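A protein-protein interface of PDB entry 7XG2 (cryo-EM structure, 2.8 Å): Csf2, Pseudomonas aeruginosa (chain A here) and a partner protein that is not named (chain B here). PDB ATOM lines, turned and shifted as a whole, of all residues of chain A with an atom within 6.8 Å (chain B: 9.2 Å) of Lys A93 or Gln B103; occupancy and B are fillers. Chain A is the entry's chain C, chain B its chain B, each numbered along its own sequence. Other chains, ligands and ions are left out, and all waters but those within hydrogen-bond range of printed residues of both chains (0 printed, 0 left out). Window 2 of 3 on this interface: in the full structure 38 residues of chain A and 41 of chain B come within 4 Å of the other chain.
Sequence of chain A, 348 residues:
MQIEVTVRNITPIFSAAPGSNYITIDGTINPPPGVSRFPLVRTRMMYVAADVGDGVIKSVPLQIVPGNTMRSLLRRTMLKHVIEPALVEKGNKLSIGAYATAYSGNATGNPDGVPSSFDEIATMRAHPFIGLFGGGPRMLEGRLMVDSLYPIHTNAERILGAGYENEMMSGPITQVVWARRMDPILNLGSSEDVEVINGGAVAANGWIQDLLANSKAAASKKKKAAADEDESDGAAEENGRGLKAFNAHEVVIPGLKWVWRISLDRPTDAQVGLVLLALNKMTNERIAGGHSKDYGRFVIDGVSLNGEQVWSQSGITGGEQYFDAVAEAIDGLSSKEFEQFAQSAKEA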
ATOM      1  N   LEU A  87     -15.773  15.451  27.810  1.00  0.00           N
ATOM      2  CA  LEU A  87     -16.646  14.864  28.822  1.00  0.00           C
ATOM      3  C   LEU A  87     -16.527  13.345  28.854  1.00  0.00           C
ATOM      4  O   LEU A  87     -16.668  12.726  29.915  1.00  0.00           O
ATOM      5  CB  LEU A  87     -18.096  15.271  28.579  1.00  0.00           C
ATOM      6  CG  LEU A  87     -18.396  16.694  29.030  1.00  0.00           C
ATOM      7  CD1 LEU A  87     -19.495  17.294  28.198  1.00  0.00           C
ATOM      8  CD2 LEU A  87     -18.709  16.741  30.486  1.00  0.00           C
ATOM      9  N   VAL A  88     -16.282  12.728  27.698  1.00  0.00           N
ATOM     10  CA  VAL A  88     -16.004  11.297  27.649  1.00  0.00           C
ATOM     11  C   VAL A  88     -14.662  10.998  28.311  1.00  0.00           C
ATOM     12  O   VAL A  88     -14.505   9.978  28.996  1.00  0.00           O
ATOM     13  CB  VAL A  88     -16.081  10.810  26.185  1.00  0.00           C
ATOM     14  CG1 VAL A  88     -15.398   9.467  25.971  1.00  0.00           C
ATOM     15  CG2 VAL A  88     -17.529  10.716  25.747  1.00  0.00           C
ATOM     16  N   GLY A  91     -15.288  10.957  31.657  1.00  0.00           N
ATOM     17  CA  GLY A  91     -16.273   9.933  31.943  1.00  0.00           C
ATOM     18  C   GLY A  91     -17.604  10.461  32.414  1.00  0.00           C
ATOM     19  O   GLY A  91     -18.373   9.717  33.029  1.00  0.00           O
ATOM     20  N   ASN A  92     -17.896  11.727  32.152  1.00  0.00           N
ATOM     21  CA  ASN A  92     -19.153  12.333  32.556  1.00  0.00           C
ATOM     22  C   ASN A  92     -20.237  12.057  31.520  1.00  0.00           C
ATOM     23  O   ASN A  92     -19.970  11.851  30.336  1.00  0.00           O
ATOM     24  CB  ASN A  92     -18.987  13.839  32.763  1.00  0.00           C
ATOM     25  CG  ASN A  92     -18.311  14.193  34.080  1.00  0.00           C
ATOM     26  OD1 ASN A  92     -18.839  14.992  34.853  1.00  0.00           O
ATOM     27  ND2 ASN A  92     -17.143  13.622  34.335  1.00  0.00           N
ATOM     28  N   LYS A  93     -21.481  12.051  31.990  1.00  0.00           N
ATOM     29  CA  LYS A  93     -22.635  11.771  31.151  1.00  0.00           C
ATOM     30  C   LYS A  93     -23.628  12.915  31.274  1.00  0.00           C
ATOM     31  O   LYS A  93     -23.589  13.692  32.231  1.00  0.00           O
ATOM     32  CB  LYS A  93     -23.317  10.448  31.535  1.00  0.00           C
ATOM     33  CG  LYS A  93     -22.372   9.265  31.646  1.00  0.00           C
ATOM     34  CD  LYS A  93     -22.951   8.175  32.526  1.00  0.00           C
ATOM     35  CE  LYS A  93     -21.853   7.295  33.099  1.00  0.00           C
ATOM     36  NZ  LYS A  93     -22.377   6.350  34.125  1.00  0.00           N
ATOM     37  N   LEU A  94     -24.517  13.012  30.294  1.00  0.00           N
ATOM     38  CA  LEU A  94     -25.551  14.031  30.275  1.00  0.00           C
ATOM     39  C   LEU A  94     -26.927  13.393  30.411  1.00  0.00           C
ATOM     40  O   LEU A  94     -27.165  12.270  29.965  1.00  0.00           O
ATOM     41  CB  LEU A  94     -25.482  14.853  28.985  1.00  0.00           C
ATOM     42  CG  LEU A  94     -24.766  16.206  29.017  1.00  0.00           C
ATOM     43  CD1 LEU A  94     -23.304  16.060  29.393  1.00  0.00           C
ATOM     44  CD2 LEU A  94     -24.910  16.900  27.674  1.00  0.00           C
ATOM     45  N   SER A  95     -27.835  14.129  31.037  1.00  0.00           N
ATOM     46  CA  SER A  95     -29.216  13.710  31.183  1.00  0.00           C
ATOM     47  C   SER A  95     -29.993  14.088  29.926  1.00  0.00           C
ATOM     48  O   SER A  95     -29.422  14.538  28.932  1.00  0.00           O
ATOM     49  CB  SER A  95     -29.825  14.337  32.438  1.00  0.00           C
ATOM     50  OG  SER A  95     -31.242  14.305  32.386  1.00  0.00           O
ATOM     51  N   ILE A  96     -31.312  13.892  29.961  1.00  0.00           N
ATOM     52  CA  ILE A  96     -32.157  14.311  28.846  1.00  0.00           C
ATOM     53  C   ILE A  96     -32.206  15.829  28.758  1.00  0.00           C
ATOM     54  O   ILE A  96     -32.108  16.410  27.669  1.00  0.00           O
ATOM     55  CB  ILE A  96     -33.569  13.712  28.991  1.00  0.00           C
ATOM     56  CG1 ILE A  96     -33.500  12.324  29.631  1.00  0.00           C
ATOM     57  CG2 ILE A  96     -34.271  13.672  27.643  1.00  0.00           C
ATOM     58  CD1 ILE A  96     -34.815  11.854  30.221  1.00  0.00           C
ATOM     59  N   ALA A  98     -30.008  18.054  30.076  1.00  0.00           N
ATOM     60  CA  ALA A  98     -28.692  18.615  29.782  1.00  0.00           C
ATOM     61  C   ALA A  98     -28.314  18.415  28.321  1.00  0.00           C
ATOM     62  O   ALA A  98     -27.651  19.271  27.725  1.00  0.00           O
ATOM     63  CB  ALA A  98     -27.639  17.993  30.697  1.00  0.00           C
ATOM     64  N   TYR A  99     -28.723  17.294  27.727  1.00  0.00           N
ATOM     65  CA  TYR A  99     -28.464  17.069  26.310  1.00  0.00           C
ATOM     66  C   TYR A  99     -29.330  17.968  25.438  1.00  0.00           C
ATOM     67  O   TYR A  99     -28.839  18.586  24.488  1.00  0.00           O
ATOM     68  CB  TYR A  99     -28.695  15.603  25.957  1.00  0.00           C
ATOM     69  CG  TYR A  99     -28.162  15.212  24.606  1.00  0.00           C
ATOM     70  CD1 TYR A  99     -26.829  14.869  24.447  1.00  0.00           C
ATOM     71  CD2 TYR A  99     -28.991  15.176  23.493  1.00  0.00           C
ATOM     72  CE1 TYR A  99     -26.334  14.509  23.219  1.00  0.00           C
ATOM     73  CE2 TYR A  99     -28.503  14.821  22.257  1.00  0.00           C
ATOM     74  CZ  TYR A  99     -27.173  14.486  22.127  1.00  0.00           C
ATOM     75  OH  TYR A  99     -26.678  14.128  20.896  1.00  0.00           O
ATOM     76  N   SER A 335     -19.685  17.714  33.578  1.00  0.00           N
ATOM     77  CA  SER A 335     -21.071  17.776  33.127  1.00  0.00           C
ATOM     78  C   SER A 335     -21.995  18.424  34.140  1.00  0.00           C
ATOM     79  O   SER A 335     -23.103  18.815  33.763  1.00  0.00           O
ATOM     80  CB  SER A 335     -21.595  16.380  32.802  1.00  0.00           C
ATOM     81  OG  SER A 335     -21.907  15.664  33.983  1.00  0.00           O
ATOM     82  N   LYS A 336     -21.561  18.560  35.400  1.00  0.00           N
ATOM     83  CA  LYS A 336     -22.441  19.072  36.447  1.00  0.00           C
ATOM     84  C   LYS A 336     -22.800  20.534  36.220  1.00  0.00           C
ATOM     85  O   LYS A 336     -23.872  20.979  36.646  1.00  0.00           O
ATOM     86  CB  LYS A 336     -21.793  18.876  37.818  1.00  0.00           C
ATOM     87  CG  LYS A 336     -20.455  19.562  37.995  1.00  0.00           C
ATOM     88  CD  LYS A 336     -20.207  19.910  39.449  1.00  0.00           C
ATOM     89  CE  LYS A 336     -21.188  20.956  39.943  1.00  0.00           C
ATOM     90  NZ  LYS A 336     -20.861  21.401  41.325  1.00  0.00           N
ATOM     91  N   GLU A 339     -25.736  20.050  33.920  1.00  0.00           N
ATOM     92  CA  GLU A 339     -26.918  19.604  34.660  1.00  0.00           C
ATOM     93  C   GLU A 339     -27.521  20.732  35.490  1.00  0.00           C
ATOM     94  O   GLU A 339     -28.746  20.891  35.530  1.00  0.00           O
ATOM     95  CB  GLU A 339     -26.596  18.409  35.566  1.00  0.00           C
ATOM     96  CG  GLU A 339     -25.650  17.350  35.015  1.00  0.00           C
ATOM     97  CD  GLU A 339     -26.334  16.293  34.156  1.00  0.00           C
ATOM     98  OE1 GLU A 339     -25.739  15.208  33.975  1.00  0.00           O
ATOM     99  OE2 GLU A 339     -27.464  16.521  33.680  1.00  0.00           O
ATOM    100  N   ALA B  93     -28.044  11.988  18.882  1.00  0.00           N
ATOM    101  CA  ALA B  93     -28.579  11.511  20.149  1.00  0.00           C
ATOM    102  C   ALA B  93     -28.585   9.996  20.224  1.00  0.00           C
ATOM    103  O   ALA B  93     -28.363   9.437  21.298  1.00  0.00           O
ATOM    104  CB  ALA B  93     -29.988  12.045  20.358  1.00  0.00           C
ATOM    105  N   HIS B  96     -24.996   9.010  20.938  1.00  0.00           N
ATOM    106  CA  HIS B  96     -24.638   9.307  22.322  1.00  0.00           C
ATOM    107  C   HIS B  96     -25.379   8.404  23.302  1.00  0.00           C
ATOM    108  O   HIS B  96     -24.853   8.078  24.372  1.00  0.00           O
ATOM    109  CB  HIS B  96     -24.922  10.776  22.620  1.00  0.00           C
ATOM    110  CG  HIS B  96     -24.092  11.722  21.812  1.00  0.00           C
ATOM    111  ND1 HIS B  96     -24.641  12.736  21.058  1.00  0.00           N
ATOM    112  CD2 HIS B  96     -22.753  11.801  21.633  1.00  0.00           C
ATOM    113  CE1 HIS B  96     -23.675  13.404  20.454  1.00  0.00           C
ATOM    114  NE2 HIS B  96     -22.521  12.857  20.787  1.00  0.00           N
ATOM    115  N   ARG B  97     -26.598   7.992  22.952  1.00  0.00           N
ATOM    116  CA  ARG B  97     -27.361   7.082  23.794  1.00  0.00           C
ATOM    117  C   ARG B  97     -26.777   5.678  23.747  1.00  0.00           C
ATOM    118  O   ARG B  97     -26.791   4.956  24.752  1.00  0.00           O
ATOM    119  CB  ARG B  97     -28.822   7.087  23.348  1.00  0.00           C
ATOM    120  CG  ARG B  97     -29.765   6.274  24.205  1.00  0.00           C
ATOM    121  CD  ARG B  97     -31.188   6.409  23.702  1.00  0.00           C
ATOM    122  NE  ARG B  97     -32.105   5.543  24.430  1.00  0.00           N
ATOM    123  CZ  ARG B  97     -32.398   4.299  24.079  1.00  0.00           C
ATOM    124  NH1 ARG B  97     -31.878   3.747  22.997  1.00  0.00           N
ATOM    125  NH2 ARG B  97     -33.231   3.591  24.836  1.00  0.00           N
ATOM    126  N   GLN B  98     -26.261   5.268  22.584  1.00  0.00           N
ATOM    127  CA  GLN B  98     -25.570   3.988  22.489  1.00  0.00           C
ATOM    128  C   GLN B  98     -24.254   4.032  23.258  1.00  0.00           C
ATOM    129  O   GLN B  98     -23.910   3.079  23.965  1.00  0.00           O
ATOM    130  CB  GLN B  98     -25.368   3.628  21.007  1.00  0.00           C
ATOM    131  CG  GLN B  98     -24.721   2.266  20.651  1.00  0.00           C
ATOM    132  CD  GLN B  98     -23.210   2.197  20.836  1.00  0.00           C
ATOM    133  OE1 GLN B  98     -22.461   2.948  20.213  1.00  0.00           O
ATOM    134  NE2 GLN B  98     -22.763   1.292  21.698  1.00  0.00           N
ATOM    135  N   SER B  99     -23.511   5.135  23.142  1.00  0.00           N
ATOM    136  CA  SER B  99     -22.231   5.236  23.834  1.00  0.00           C
ATOM    137  C   SER B  99     -22.389   5.533  25.318  1.00  0.00           C
ATOM    138  O   SER B  99     -21.424   5.379  26.073  1.00  0.00           O
ATOM    139  CB  SER B  99     -21.362   6.310  23.184  1.00  0.00           C
ATOM    140  OG  SER B  99     -20.162   6.501  23.914  1.00  0.00           O
ATOM    141  N   GLY B 100     -23.574   5.954  25.754  1.00  0.00           N
ATOM    142  CA  GLY B 100     -23.816   6.252  27.146  1.00  0.00           C
ATOM    143  C   GLY B 100     -23.487   7.665  27.572  1.00  0.00           C
ATOM    144  O   GLY B 100     -23.615   7.977  28.762  1.00  0.00           O
ATOM    145  N   TYR B 101     -23.057   8.526  26.645  1.00  0.00           N
ATOM    146  CA  TYR B 101     -22.821   9.924  26.991  1.00  0.00           C
ATOM    147  C   TYR B 101     -24.134  10.642  27.269  1.00  0.00           C
ATOM    148  O   TYR B 101     -24.182  11.548  28.107  1.00  0.00           O
ATOM    149  CB  TYR B 101     -22.014  10.605  25.872  1.00  0.00           C
ATOM    150  CG  TYR B 101     -22.093  12.124  25.791  1.00  0.00           C
ATOM    151  CD1 TYR B 101     -21.148  12.913  26.434  1.00  0.00           C
ATOM    152  CD2 TYR B 101     -23.041  12.763  24.989  1.00  0.00           C
ATOM    153  CE1 TYR B 101     -21.193  14.292  26.352  1.00  0.00           C
ATOM    154  CE2 TYR B 101     -23.093  14.140  24.903  1.00  0.00           C
ATOM    155  CZ  TYR B 101     -22.163  14.897  25.581  1.00  0.00           C
ATOM    156  OH  TYR B 101     -22.204  16.267  25.492  1.00  0.00           O
ATOM    157  N   LEU B 102     -25.200  10.257  26.579  1.00  0.00           N
ATOM    158  CA  LEU B 102     -26.544  10.734  26.868  1.00  0.00           C
ATOM    159  C   LEU B 102     -27.272   9.646  27.645  1.00  0.00           C
ATOM    160  O   LEU B 102     -27.362   8.503  27.185  1.00  0.00           O
ATOM    161  CB  LEU B 102     -27.287  11.089  25.579  1.00  0.00           C
ATOM    162  CG  LEU B 102     -28.814  11.021  25.511  1.00  0.00           C
ATOM    163  CD1 LEU B 102     -29.483  12.043  26.412  1.00  0.00           C
ATOM    164  CD2 LEU B 102     -29.278  11.203  24.080  1.00  0.00           C
ATOM    165  N   GLN B 103     -27.774   9.998  28.827  1.00  0.00           N
ATOM    166  CA  GLN B 103     -28.499   9.051  29.672  1.00  0.00           C
ATOM    167  C   GLN B 103     -29.999   9.197  29.417  1.00  0.00           C
ATOM    168  O   GLN B 103     -30.738   9.845  30.159  1.00  0.00           O
ATOM    169  CB  GLN B 103     -28.148   9.266  31.137  1.00  0.00           C
ATOM    170  CG  GLN B 103     -26.746   8.818  31.501  1.00  0.00           C
ATOM    171  CD  GLN B 103     -26.572   7.317  31.409  1.00  0.00           C
ATOM    172  OE1 GLN B 103     -25.556   6.828  30.915  1.00  0.00           O
ATOM    173  NE2 GLN B 103     -27.563   6.575  31.888  1.00  0.00           N
ATOM    174  N   LEU B 104     -30.437   8.580  28.325  1.00  0.00           N
ATOM    175  CA  LEU B 104     -31.835   8.590  27.914  1.00  0.00           C
ATOM    176  C   LEU B 104     -32.339   7.155  27.888  1.00  0.00           C
ATOM    177  O   LEU B 104     -31.838   6.329  27.119  1.00  0.00           O
ATOM    178  CB  LEU B 104     -31.998   9.252  26.550  1.00  0.00           C
ATOM    179  CG  LEU B 104     -33.402   9.246  25.951  1.00  0.00           C
ATOM    180  CD1 LEU B 104     -34.384   9.982  26.836  1.00  0.00           C
ATOM    181  CD2 LEU B 104     -33.361   9.864  24.583  1.00  0.00           C
ATOM    182  N   ARG B 105     -33.324   6.859  28.735  1.00  0.00           N
ATOM    183  CA  ARG B 105     -33.920   5.530  28.757  1.00  0.00           C
ATOM    184  C   ARG B 105     -34.886   5.324  27.598  1.00  0.00           C
ATOM    185  O   ARG B 105     -35.067   4.189  27.143  1.00  0.00           O
ATOM    186  CB  ARG B 105     -34.625   5.305  30.097  1.00  0.00           C
ATOM    187  CG  ARG B 105     -35.031   3.867  30.384  1.00  0.00           C
ATOM    188  CD  ARG B 105     -35.214   3.631  31.878  1.00  0.00           C
ATOM    189  NE  ARG B 105     -36.118   4.601  32.487  1.00  0.00           N
ATOM    190  CZ  ARG B 105     -37.442   4.544  32.429  1.00  0.00           C
ATOM    191  NH1 ARG B 105     -38.068   3.562  31.801  1.00  0.00           N
ATOM    192  NH2 ARG B 105     -38.158   5.497  33.020  1.00  0.00           N
ATOM    193  N   ALA B 106     -35.499   6.401  27.105  1.00  0.00           N
ATOM    194  CA  ALA B 106     -36.487   6.294  26.039  1.00  0.00           C
ATOM    195  C   ALA B 106     -35.829   5.896  24.725  1.00  0.00           C
ATOM    196  O   ALA B 106     -34.820   6.478  24.318  1.00  0.00           O
ATOM    197  CB  ALA B 106     -37.229   7.619  25.876  1.00  0.00           C
ATOM    198  N   PHE B 116     -36.932  16.031  21.329  1.00  0.00           N
ATOM    199  CA  PHE B 116     -36.632  15.826  19.921  1.00  0.00           C
ATOM    200  C   PHE B 116     -37.739  16.356  19.028  1.00  0.00           C
ATOM    201  O   PHE B 116     -37.925  15.861  17.913  1.00  0.00           O
ATOM    202  CB  PHE B 116     -36.387  14.346  19.651  1.00  0.00           C
ATOM    203  CG  PHE B 116     -35.390  13.744  20.577  1.00  0.00           C
ATOM    204  CD1 PHE B 116     -34.041  13.934  20.364  1.00  0.00           C
ATOM    205  CD2 PHE B 116     -35.798  13.009  21.677  1.00  0.00           C
ATOM    206  CE1 PHE B 116     -33.120  13.401  21.224  1.00  0.00           C
ATOM    207  CE2 PHE B 116     -34.875  12.470  22.539  1.00  0.00           C
ATOM    208  CZ  PHE B 116     -33.532  12.667  22.311  1.00  0.00           C
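The backbone carbonyl oxygen (O) of Leu B104 lies within hydrogen-bond range of the guanidinium group (NE) of Arg B97 (2.8 Å). The backbone carbonyl oxygen (O) of Lys A93 is in hydrogen-bond range of the side-chain hydroxyl (OG) of Ser A335, at 3.1 Å. The backbone carbonyl oxygen (O) of His B96 sits at hydrogen-bond distance from the backbone NH (N) of Leu B102 (3.1 Å). O of His B96 sits at hydrogen-bond distance from N of Tyr B101 (2.9 Å). The backbone carbonyl oxygen (O) of Gly B100 lies close to the side-chain amide oxygen (OE1) of Gln B103, 3.1 Å away. The backbone carbonyl oxygen (O) of Leu A87 is in hydrogen-bond range of the backbone NH (N) of Asn A92 (2.7 Å).
Hydrophobic or aromatic side chains of chain B within 4 Å of the printed part of chain A: Ala B93, His B96, Tyr B101, Leu B102 and Leu B104. Printed residues of chain A that touch a printed residue of chain B: Leu A87, Lys A93, Leu A94, Ser A95, Ile A96 and Tyr A99.
OH of Tyr A99 sits at hydrogen-bond distance from ND1 of His B96 (2.5 Å). The backbone NH of Gln B103 sits at hydrogen-bond distance from the backbone carbonyl oxygen of Leu A94. The backbone carbonyl oxygen (O) of Tyr B101 sits at hydrogen-bond distance from the backbone NH (N) of Leu A94, at 2.7 Å. N of Ala B93 lies within hydrogen-bond range of OH of Tyr A99 (3.2 Å).
Of the printed residues of chain B, Ser A95 touches Leu B102 (3.5 Å). Printed residues of chain B within 4 Å of Tyr A99: Ala B93, His B96, Tyr B101 and Leu B102. Printed residues of chain A within 4 Å of Tyr B101: Leu A87, Lys A93, Leu A94 and Tyr A99. Of the printed residues of chain A, Leu B102 touches Leu A94 (3.5 Å), Ser A95 (3.5 Å) and Tyr A99 (3.7 Å). Gln B103 touches just these residues of chain A: Lys A93, Leu A94 and Ile A96. Printed residues of chain A within 4 Å of Leu B104: Ile A96 (3.8 Å).
Among the printed residues, merely in contact across the chains: Leu A87 with Tyr B101, Lys A93 with Gly B100, Lys A93 with Tyr B101, Lys A93 with Gln B103, Leu A94 with Leu B102, Ser A95 with Leu B102, Ile A96 with Gln B103, Ile A96 with Leu B104, Tyr A99 with Tyr B101 and Tyr A99 with Leu B102.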
